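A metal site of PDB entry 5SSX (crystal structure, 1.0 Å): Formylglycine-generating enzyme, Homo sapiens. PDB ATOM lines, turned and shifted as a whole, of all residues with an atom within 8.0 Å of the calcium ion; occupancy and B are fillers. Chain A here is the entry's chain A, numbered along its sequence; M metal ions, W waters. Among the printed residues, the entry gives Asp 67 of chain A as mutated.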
ATOM      1  N   ASP A  67      12.350 -28.613  24.085  1.00  0.00           N
ATOM      2  CA  ASP A  67      11.802 -29.668  23.233  1.00  0.00           C
ATOM      3  C   ASP A  67      11.735 -30.965  24.011  1.00  0.00           C
ATOM      4  O   ASP A  67      12.519 -31.188  24.934  1.00  0.00           O
ATOM      5  CB  ASP A  67      12.648 -29.902  22.004  1.00  0.00           C
ATOM      6  CG  ASP A  67      12.472 -28.848  20.970  1.00  0.00           C
ATOM      7  OD1 ASP A  67      11.465 -28.149  21.001  1.00  0.00           O
ATOM      8  OD2 ASP A  67      13.336 -28.727  20.109  1.00  0.00           O
ATOM      9  N   PRO A 142      16.873 -33.546  21.716  1.00  0.00           N
ATOM     10  CA  PRO A 142      15.472 -33.614  21.277  1.00  0.00           C
ATOM     11  C   PRO A 142      15.189 -34.944  20.601  1.00  0.00           C
ATOM     12  O   PRO A 142      15.986 -35.440  19.821  1.00  0.00           O
ATOM     13  CB  PRO A 142      15.352 -32.457  20.279  1.00  0.00           C
ATOM     14  CG  PRO A 142      16.727 -32.103  19.957  1.00  0.00           C
ATOM     15  CD  PRO A 142      17.618 -32.466  21.050  1.00  0.00           C
ATOM     16  N   TRP A 168       3.323 -20.287  19.104  1.00  0.00           N
ATOM     17  CA  TRP A 168       4.727 -20.627  18.946  1.00  0.00           C
ATOM     18  C   TRP A 168       5.533 -19.385  18.590  1.00  0.00           C
ATOM     19  O   TRP A 168       6.549 -19.107  19.205  1.00  0.00           O
ATOM     20  CB  TRP A 168       4.852 -21.733  17.869  1.00  0.00           C
ATOM     21  CG  TRP A 168       6.240 -22.294  17.814  1.00  0.00           C
ATOM     22  CD1 TRP A 168       6.661 -23.466  18.374  1.00  0.00           C
ATOM     23  CD2 TRP A 168       7.395 -21.689  17.234  1.00  0.00           C
ATOM     24  NE1 TRP A 168       8.003 -23.629  18.187  1.00  0.00           N
ATOM     25  CE2 TRP A 168       8.475 -22.557  17.479  1.00  0.00           C
ATOM     26  CE3 TRP A 168       7.616 -20.517  16.511  1.00  0.00           C
ATOM     27  CZ2 TRP A 168       9.765 -22.252  17.073  1.00  0.00           C
ATOM     28  CZ3 TRP A 168       8.908 -20.228  16.110  1.00  0.00           C
ATOM     29  CH2 TRP A 168       9.961 -21.092  16.423  1.00  0.00           C
ATOM     30  N   CYS A 172       8.421 -17.631  20.676  1.00  0.00           N
ATOM     31  CA  CYS A 172       9.752 -17.527  20.086  1.00  0.00           C
ATOM     32  C   CYS A 172      10.298 -16.106  20.229  1.00  0.00           C
ATOM     33  O   CYS A 172      11.468 -15.894  20.570  1.00  0.00           O
ATOM     34  CB  CYS A 172       9.647 -17.906  18.598  1.00  0.00           C
ATOM     35  SG  CYS A 172      11.148 -17.889  17.655  1.00  0.00           S
ATOM     36  N   ALA A 195      22.244 -20.146  19.185  1.00  0.00           N
ATOM     37  CA  ALA A 195      21.417 -21.232  18.668  1.00  0.00           C
ATOM     38  C   ALA A 195      22.302 -22.178  17.885  1.00  0.00           C
ATOM     39  O   ALA A 195      23.383 -21.794  17.373  1.00  0.00           O
ATOM     40  CB  ALA A 195      20.307 -20.715  17.768  1.00  0.00           C
ATOM     41  N   ASN A 196      21.847 -23.418  17.755  1.00  0.00           N
ATOM     42  CA  ASN A 196      22.533 -24.471  17.038  1.00  0.00           C
ATOM     43  C   ASN A 196      22.038 -24.529  15.605  1.00  0.00           C
ATOM     44  O   ASN A 196      20.968 -25.087  15.324  1.00  0.00           O
ATOM     45  CB  ASN A 196      22.287 -25.791  17.744  1.00  0.00           C
ATOM     46  CG  ASN A 196      22.965 -26.950  17.039  1.00  0.00           C
ATOM     47  OD1 ASN A 196      23.915 -26.752  16.270  1.00  0.00           O
ATOM     48  ND2 ASN A 196      22.517 -28.151  17.325  1.00  0.00           N
ATOM     49  N   TYR A 229      14.283 -22.628  25.627  1.00  0.00           N
ATOM     50  CA  TYR A 229      15.563 -23.084  25.120  1.00  0.00           C
ATOM     51  C   TYR A 229      15.416 -23.672  23.725  1.00  0.00           C
ATOM     52  O   TYR A 229      14.504 -24.463  23.463  1.00  0.00           O
ATOM     53  CB  TYR A 229      16.170 -24.130  26.054  1.00  0.00           C
ATOM     54  CG  TYR A 229      16.564 -23.558  27.380  1.00  0.00           C
ATOM     55  CD1 TYR A 229      15.634 -23.341  28.367  1.00  0.00           C
ATOM     56  CD2 TYR A 229      17.879 -23.198  27.634  1.00  0.00           C
ATOM     57  CE1 TYR A 229      15.987 -22.807  29.585  1.00  0.00           C
ATOM     58  CE2 TYR A 229      18.247 -22.651  28.850  1.00  0.00           C
ATOM     59  CZ  TYR A 229      17.301 -22.448  29.817  1.00  0.00           C
ATOM     60  OH  TYR A 229      17.680 -21.884  31.023  1.00  0.00           O
ATOM     61  N   ASN A 230      16.329 -23.285  22.854  1.00  0.00           N
ATOM     62  CA  ASN A 230      16.422 -23.789  21.482  1.00  0.00           C
ATOM     63  C   ASN A 230      15.118 -23.636  20.718  1.00  0.00           C
ATOM     64  O   ASN A 230      14.722 -24.495  19.961  1.00  0.00           O
ATOM     65  CB  ASN A 230      16.945 -25.212  21.437  1.00  0.00           C
ATOM     66  CG  ASN A 230      18.312 -25.297  22.052  1.00  0.00           C
ATOM     67  OD1 ASN A 230      19.272 -24.762  21.514  1.00  0.00           O
ATOM     68  ND2 ASN A 230      18.390 -25.849  23.244  1.00  0.00           N
ATOM     69  N   ILE A 231      14.481 -22.488  20.898  1.00  0.00           N
ATOM     70  CA  ILE A 231      13.243 -22.227  20.177  1.00  0.00           C
ATOM     71  C   ILE A 231      13.540 -22.043  18.694  1.00  0.00           C
ATOM     72  O   ILE A 231      12.780 -22.532  17.842  1.00  0.00           O
ATOM     73  CB  ILE A 231      12.433 -21.094  20.835  1.00  0.00           C
ATOM     74  CG1 ILE A 231      10.988 -21.080  20.306  1.00  0.00           C
ATOM     75  CG2 ILE A 231      13.054 -19.729  20.694  1.00  0.00           C
ATOM     76  CD1 ILE A 231      10.187 -22.267  20.701  1.00  0.00           C
ATOM     77  N   VAL A 232      14.657 -21.396  18.334  1.00  0.00           N
ATOM     78  CA  VAL A 232      15.170 -21.483  16.980  1.00  0.00           C
ATOM     79  C   VAL A 232      16.417 -22.343  16.949  1.00  0.00           C
ATOM     80  O   VAL A 232      17.166 -22.425  17.909  1.00  0.00           O
ATOM     81  CB  VAL A 232      15.407 -20.140  16.251  1.00  0.00           C
ATOM     82  CG1 VAL A 232      14.124 -19.364  16.202  1.00  0.00           C
ATOM     83  CG2 VAL A 232      16.539 -19.333  16.871  1.00  0.00           C
ATOM     84  N   GLY A 233      16.635 -22.972  15.813  1.00  0.00           N
ATOM     85  CA  GLY A 233      17.723 -23.922  15.657  1.00  0.00           C
ATOM     86  C   GLY A 233      17.457 -25.237  16.350  1.00  0.00           C
ATOM     87  O   GLY A 233      16.392 -25.475  16.914  1.00  0.00           O
ATOM     88  N   ASN A 234      18.460 -26.108  16.276  1.00  0.00           N
ATOM     89  CA  ASN A 234      18.467 -27.419  16.931  1.00  0.00           C
ATOM     90  C   ASN A 234      17.575 -28.385  16.175  1.00  0.00           C
ATOM     91  O   ASN A 234      18.083 -29.173  15.368  1.00  0.00           O
ATOM     92  CB  ASN A 234      18.229 -27.360  18.448  1.00  0.00           C
ATOM     93  CG  ASN A 234      19.004 -28.422  19.187  1.00  0.00           C
ATOM     94  OD1 ASN A 234      20.062 -28.832  18.715  1.00  0.00           O
ATOM     95  ND2 ASN A 234      18.510 -28.861  20.337  1.00  0.00           N
ATOM     96  N   ALA A 235      16.276 -28.348  16.405  1.00  0.00           N
ATOM     97  CA  ALA A 235      15.315 -29.182  15.676  1.00  0.00           C
ATOM     98  C   ALA A 235      14.107 -28.349  15.312  1.00  0.00           C
ATOM     99  O   ALA A 235      13.673 -27.508  16.097  1.00  0.00           O
ATOM    100  CB  ALA A 235      14.878 -30.365  16.525  1.00  0.00           C
ATOM    101  N   TRP A 236      13.530 -28.590  14.145  1.00  0.00           N
ATOM    102  CA  TRP A 236      12.233 -28.023  13.807  1.00  0.00           C
ATOM    103  C   TRP A 236      11.215 -28.476  14.833  1.00  0.00           C
ATOM    104  O   TRP A 236      11.346 -29.530  15.456  1.00  0.00           O
ATOM    105  CB  TRP A 236      11.778 -28.535  12.445  1.00  0.00           C
ATOM    106  CG  TRP A 236      12.439 -27.897  11.273  1.00  0.00           C
ATOM    107  CD1 TRP A 236      13.521 -28.350  10.564  1.00  0.00           C
ATOM    108  CD2 TRP A 236      12.038 -26.693  10.647  1.00  0.00           C
ATOM    109  NE1 TRP A 236      13.798 -27.475   9.552  1.00  0.00           N
ATOM    110  CE2 TRP A 236      12.891 -26.448   9.573  1.00  0.00           C
ATOM    111  CE3 TRP A 236      11.015 -25.788  10.910  1.00  0.00           C
ATOM    112  CZ2 TRP A 236      12.746 -25.324   8.742  1.00  0.00           C
ATOM    113  CZ3 TRP A 236      10.863 -24.700  10.080  1.00  0.00           C
ATOM    114  CH2 TRP A 236      11.730 -24.481   9.037  1.00  0.00           C
ATOM    115  N   GLU A 237      10.138 -27.714  14.945  1.00  0.00           N
ATOM    116  CA  GLU A 237       9.087 -27.993  15.917  1.00  0.00           C
ATOM    117  C   GLU A 237       7.723 -27.973  15.246  1.00  0.00           C
ATOM    118  O   GLU A 237       7.317 -26.978  14.654  1.00  0.00           O
ATOM    119  CB  GLU A 237       9.146 -27.015  17.071  1.00  0.00           C
ATOM    120  CG  GLU A 237      10.488 -27.125  17.777  1.00  0.00           C
ATOM    121  CD  GLU A 237      10.704 -26.139  18.906  1.00  0.00           C
ATOM    122  OE1 GLU A 237       9.750 -25.505  19.366  1.00  0.00           O
ATOM    123  OE2 GLU A 237      11.867 -26.065  19.395  1.00  0.00           O
ATOM    124  N   LYS A 267       8.054 -24.935  12.713  1.00  0.00           N
ATOM    125  CA  LYS A 267       8.704 -23.670  12.999  1.00  0.00           C
ATOM    126  C   LYS A 267      10.100 -23.875  13.563  1.00  0.00           C
ATOM    127  O   LYS A 267      10.407 -24.879  14.190  1.00  0.00           O
ATOM    128  CB  LYS A 267       7.892 -22.867  14.021  1.00  0.00           C
ATOM    129  CG  LYS A 267       6.508 -22.438  13.525  1.00  0.00           C
ATOM    130  CD  LYS A 267       6.507 -21.303  12.517  1.00  0.00           C
ATOM    131  CE  LYS A 267       6.525 -19.944  13.195  1.00  0.00           C
ATOM    132  NZ  LYS A 267       6.273 -18.853  12.182  1.00  0.00           N
ATOM    133  N   GLY A 268      10.930 -22.861  13.369  1.00  0.00           N
ATOM    134  CA  GLY A 268      12.131 -22.661  14.144  1.00  0.00           C
ATOM    135  C   GLY A 268      13.446 -23.075  13.513  1.00  0.00           C
ATOM    136  O   GLY A 268      14.499 -22.685  14.015  1.00  0.00           O
ATOM    137  N   GLY A 269      13.436 -23.851  12.463  1.00  0.00           N
ATOM    138  CA  GLY A 269      14.676 -24.301  11.873  1.00  0.00           C
ATOM    139  C   GLY A 269      15.366 -25.353  12.727  1.00  0.00           C
ATOM    140  O   GLY A 269      14.843 -25.862  13.697  1.00  0.00           O
ATOM    141  N   SER A 270      16.584 -25.709  12.300  1.00  0.00           N
ATOM    142  CA  SER A 270      17.280 -26.845  12.888  1.00  0.00           C
ATOM    143  C   SER A 270      18.786 -26.622  12.821  1.00  0.00           C
ATOM    144  O   SER A 270      19.285 -25.624  12.279  1.00  0.00           O
ATOM    145  CB  SER A 270      16.956 -28.164  12.187  1.00  0.00           C
ATOM    146  OG  SER A 270      17.656 -28.290  10.960  1.00  0.00           O
ATOM    147  N   TYR A 271      19.528 -27.613  13.303  1.00  0.00           N
ATOM    148  CA  TYR A 271      20.982 -27.638  13.241  1.00  0.00           C
ATOM    149  C   TYR A 271      21.519 -27.596  11.819  1.00  0.00           C
ATOM    150  O   TYR A 271      22.709 -27.328  11.643  1.00  0.00           O
ATOM    151  CB  TYR A 271      21.494 -28.861  13.974  1.00  0.00           C
ATOM    152  CG  TYR A 271      21.278 -30.201  13.314  1.00  0.00           C
ATOM    153  CD1 TYR A 271      22.095 -30.620  12.293  1.00  0.00           C
ATOM    154  CD2 TYR A 271      20.287 -31.057  13.769  1.00  0.00           C
ATOM    155  CE1 TYR A 271      21.969 -31.873  11.715  1.00  0.00           C
ATOM    156  CE2 TYR A 271      20.146 -32.324  13.192  1.00  0.00           C
ATOM    157  CZ  TYR A 271      21.006 -32.715  12.186  1.00  0.00           C
ATOM    158  OH  TYR A 271      20.898 -33.970  11.635  1.00  0.00           O
ATOM    159  N   ARG A 280      15.882 -20.163   8.045  1.00  0.00           N
ATOM    160  CA  ARG A 280      14.616 -20.416   8.717  1.00  0.00           C
ATOM    161  C   ARG A 280      14.744 -20.519  10.228  1.00  0.00           C
ATOM    162  O   ARG A 280      13.845 -21.009  10.892  1.00  0.00           O
ATOM    163  CB  ARG A 280      13.869 -21.591   8.105  1.00  0.00           C
ATOM    164  CG  ARG A 280      13.434 -21.324   6.656  1.00  0.00           C
ATOM    165  CD  ARG A 280      12.515 -22.387   6.138  1.00  0.00           C
ATOM    166  NE  ARG A 280      11.973 -22.114   4.823  1.00  0.00           N
ATOM    167  CZ  ARG A 280      12.574 -22.405   3.682  1.00  0.00           C
ATOM    168  NH1 ARG A 280      13.773 -22.956   3.647  1.00  0.00           N
ATOM    169  NH2 ARG A 280      11.954 -22.139   2.540  1.00  0.00           N
ATOM    170  N   TYR A 281      15.809 -19.951  10.773  1.00  0.00           N
ATOM    171  CA  TYR A 281      16.031 -19.826  12.211  1.00  0.00           C
ATOM    172  C   TYR A 281      15.597 -18.459  12.719  1.00  0.00           C
ATOM    173  O   TYR A 281      16.141 -17.913  13.664  1.00  0.00           O
ATOM    174  CB  TYR A 281      17.480 -20.146  12.570  1.00  0.00           C
ATOM    175  CG  TYR A 281      18.500 -19.407  11.728  1.00  0.00           C
ATOM    176  CD1 TYR A 281      18.940 -19.939  10.525  1.00  0.00           C
ATOM    177  CD2 TYR A 281      19.015 -18.180  12.110  1.00  0.00           C
ATOM    178  CE1 TYR A 281      19.846 -19.280   9.735  1.00  0.00           C
ATOM    179  CE2 TYR A 281      19.938 -17.511  11.306  1.00  0.00           C
ATOM    180  CZ  TYR A 281      20.363 -18.070  10.123  1.00  0.00           C
ATOM    181  OH  TYR A 281      21.274 -17.431   9.324  1.00  0.00           O
ATOM    182  N   ASN A 297      15.729 -34.038  11.664  1.00  0.00           N
ATOM    183  CA  ASN A 297      15.902 -32.694  12.174  1.00  0.00           C
ATOM    184  C   ASN A 297      14.603 -32.089  12.681  1.00  0.00           C
ATOM    185  O   ASN A 297      14.496 -30.862  12.768  1.00  0.00           O
ATOM    186  CB  ASN A 297      16.548 -31.768  11.158  1.00  0.00           C
ATOM    187  CG  ASN A 297      15.614 -31.464  10.029  1.00  0.00           C
ATOM    188  OD1 ASN A 297      14.599 -32.157   9.840  1.00  0.00           O
ATOM    189  ND2 ASN A 297      15.943 -30.424   9.243  1.00  0.00           N
ATOM    190  N   GLY A 299      11.452 -32.326  15.571  1.00  0.00           N
ATOM    191  CA  GLY A 299      10.931 -32.682  16.872  1.00  0.00           C
ATOM    192  C   GLY A 299       9.745 -31.816  17.241  1.00  0.00           C
ATOM    193  O   GLY A 299       8.980 -31.377  16.382  1.00  0.00           O
ATOM    194  N   PHE A 300       9.591 -31.543  18.538  1.00  0.00           N
ATOM    195  CA  PHE A 300       8.448 -30.756  19.010  1.00  0.00           C
ATOM    196  C   PHE A 300       8.613 -30.412  20.475  1.00  0.00           C
ATOM    197  O   PHE A 300       9.369 -31.051  21.214  1.00  0.00           O
ATOM    198  CB  PHE A 300       7.105 -31.485  18.814  1.00  0.00           C
ATOM    199  CG  PHE A 300       6.966 -32.734  19.647  1.00  0.00           C
ATOM    200  CD1 PHE A 300       7.634 -33.882  19.310  1.00  0.00           C
ATOM    201  CD2 PHE A 300       6.134 -32.753  20.754  1.00  0.00           C
ATOM    202  CE1 PHE A 300       7.517 -35.029  20.068  1.00  0.00           C
ATOM    203  CE2 PHE A 300       5.988 -33.915  21.496  1.00  0.00           C
ATOM    204  CZ  PHE A 300       6.691 -35.042  21.174  1.00  0.00           C
ATOM    205  N   ARG A 301       7.816 -29.439  20.895  1.00  0.00           N
ATOM    206  CA  ARG A 301       7.554 -29.134  22.290  1.00  0.00           C
ATOM    207  C   ARG A 301       6.048 -28.987  22.480  1.00  0.00           C
ATOM    208  O   ARG A 301       5.311 -28.744  21.546  1.00  0.00           O
ATOM    209  CB  ARG A 301       8.285 -27.880  22.765  1.00  0.00           C
ATOM    210  CG  ARG A 301       7.702 -26.549  22.287  1.00  0.00           C
ATOM    211  CD  ARG A 301       8.509 -25.371  22.797  1.00  0.00           C
ATOM    212  NE  ARG A 301       9.821 -25.321  22.174  1.00  0.00           N
ATOM    213  CZ  ARG A 301      10.957 -25.052  22.784  1.00  0.00           C
ATOM    214  NH1 ARG A 301      11.012 -24.794  24.072  1.00  0.00           N
ATOM    215  NH2 ARG A 301      12.064 -25.014  22.058  1.00  0.00           N
HETATM  216 CA    CA M   1      13.796 -25.234  17.552  1.00  0.00          CA
HETATM  217  O   HOH W   1      14.942 -27.158  19.019  1.00  0.00           O
HETATM  218  O   HOH W   2      13.050 -24.891  15.688  1.00  0.00           O
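The backbone carbonyl oxygen (O) of Gly 268 is in hydrogen-bond range of the backbone NH (N) of Gly 233, at 2.8 Å.
O of Asn 230 sits close to NH2 of Arg 301, at 3.4 Å.
The side-chain carboxylate (OE2) of Glu 237 sits close to the side-chain carboxylate (OD1) of Asp 67 (2.7 Å).
The backbone carbonyl oxygen of Glu 237 is in hydrogen-bond range of the backbone NH of Lys 267.
NE of Arg 301 is in salt-bridge range of OE1 of Glu 237 (2.8 Å).
OE1 of Glu 237 lies within hydrogen-bond range of NE1 of Trp 168 (2.8 Å).
Val 232 touches the calcium ion.
Of the 26 residues printed, 6 come within 4 Å of the calcium ion.
The nearest printed residue that does not touch the calcium ion is Gly 269 (4.04 Å).
Water W2 binds the calcium ion (2.0 Å).
Water W1 is bound to the calcium ion (2.7 Å).
The calcium ion is bound by O of Gly 233 (2.7 Å).
O of Asn 230 is bound to the calcium ion (2.7 Å).
The calcium ion is bound by the backbone carbonyl oxygen (O) of Ala 235, 2.7 Å away.
OE2 of Glu 237 binds the calcium ion.
O of Ile 231 binds the calcium ion, at 2.9 Å.
Water W1 lies within hydrogen-bond range of OD2 of Asp 67 (2.5 Å) and N of Ala 235 (3.2 Å).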
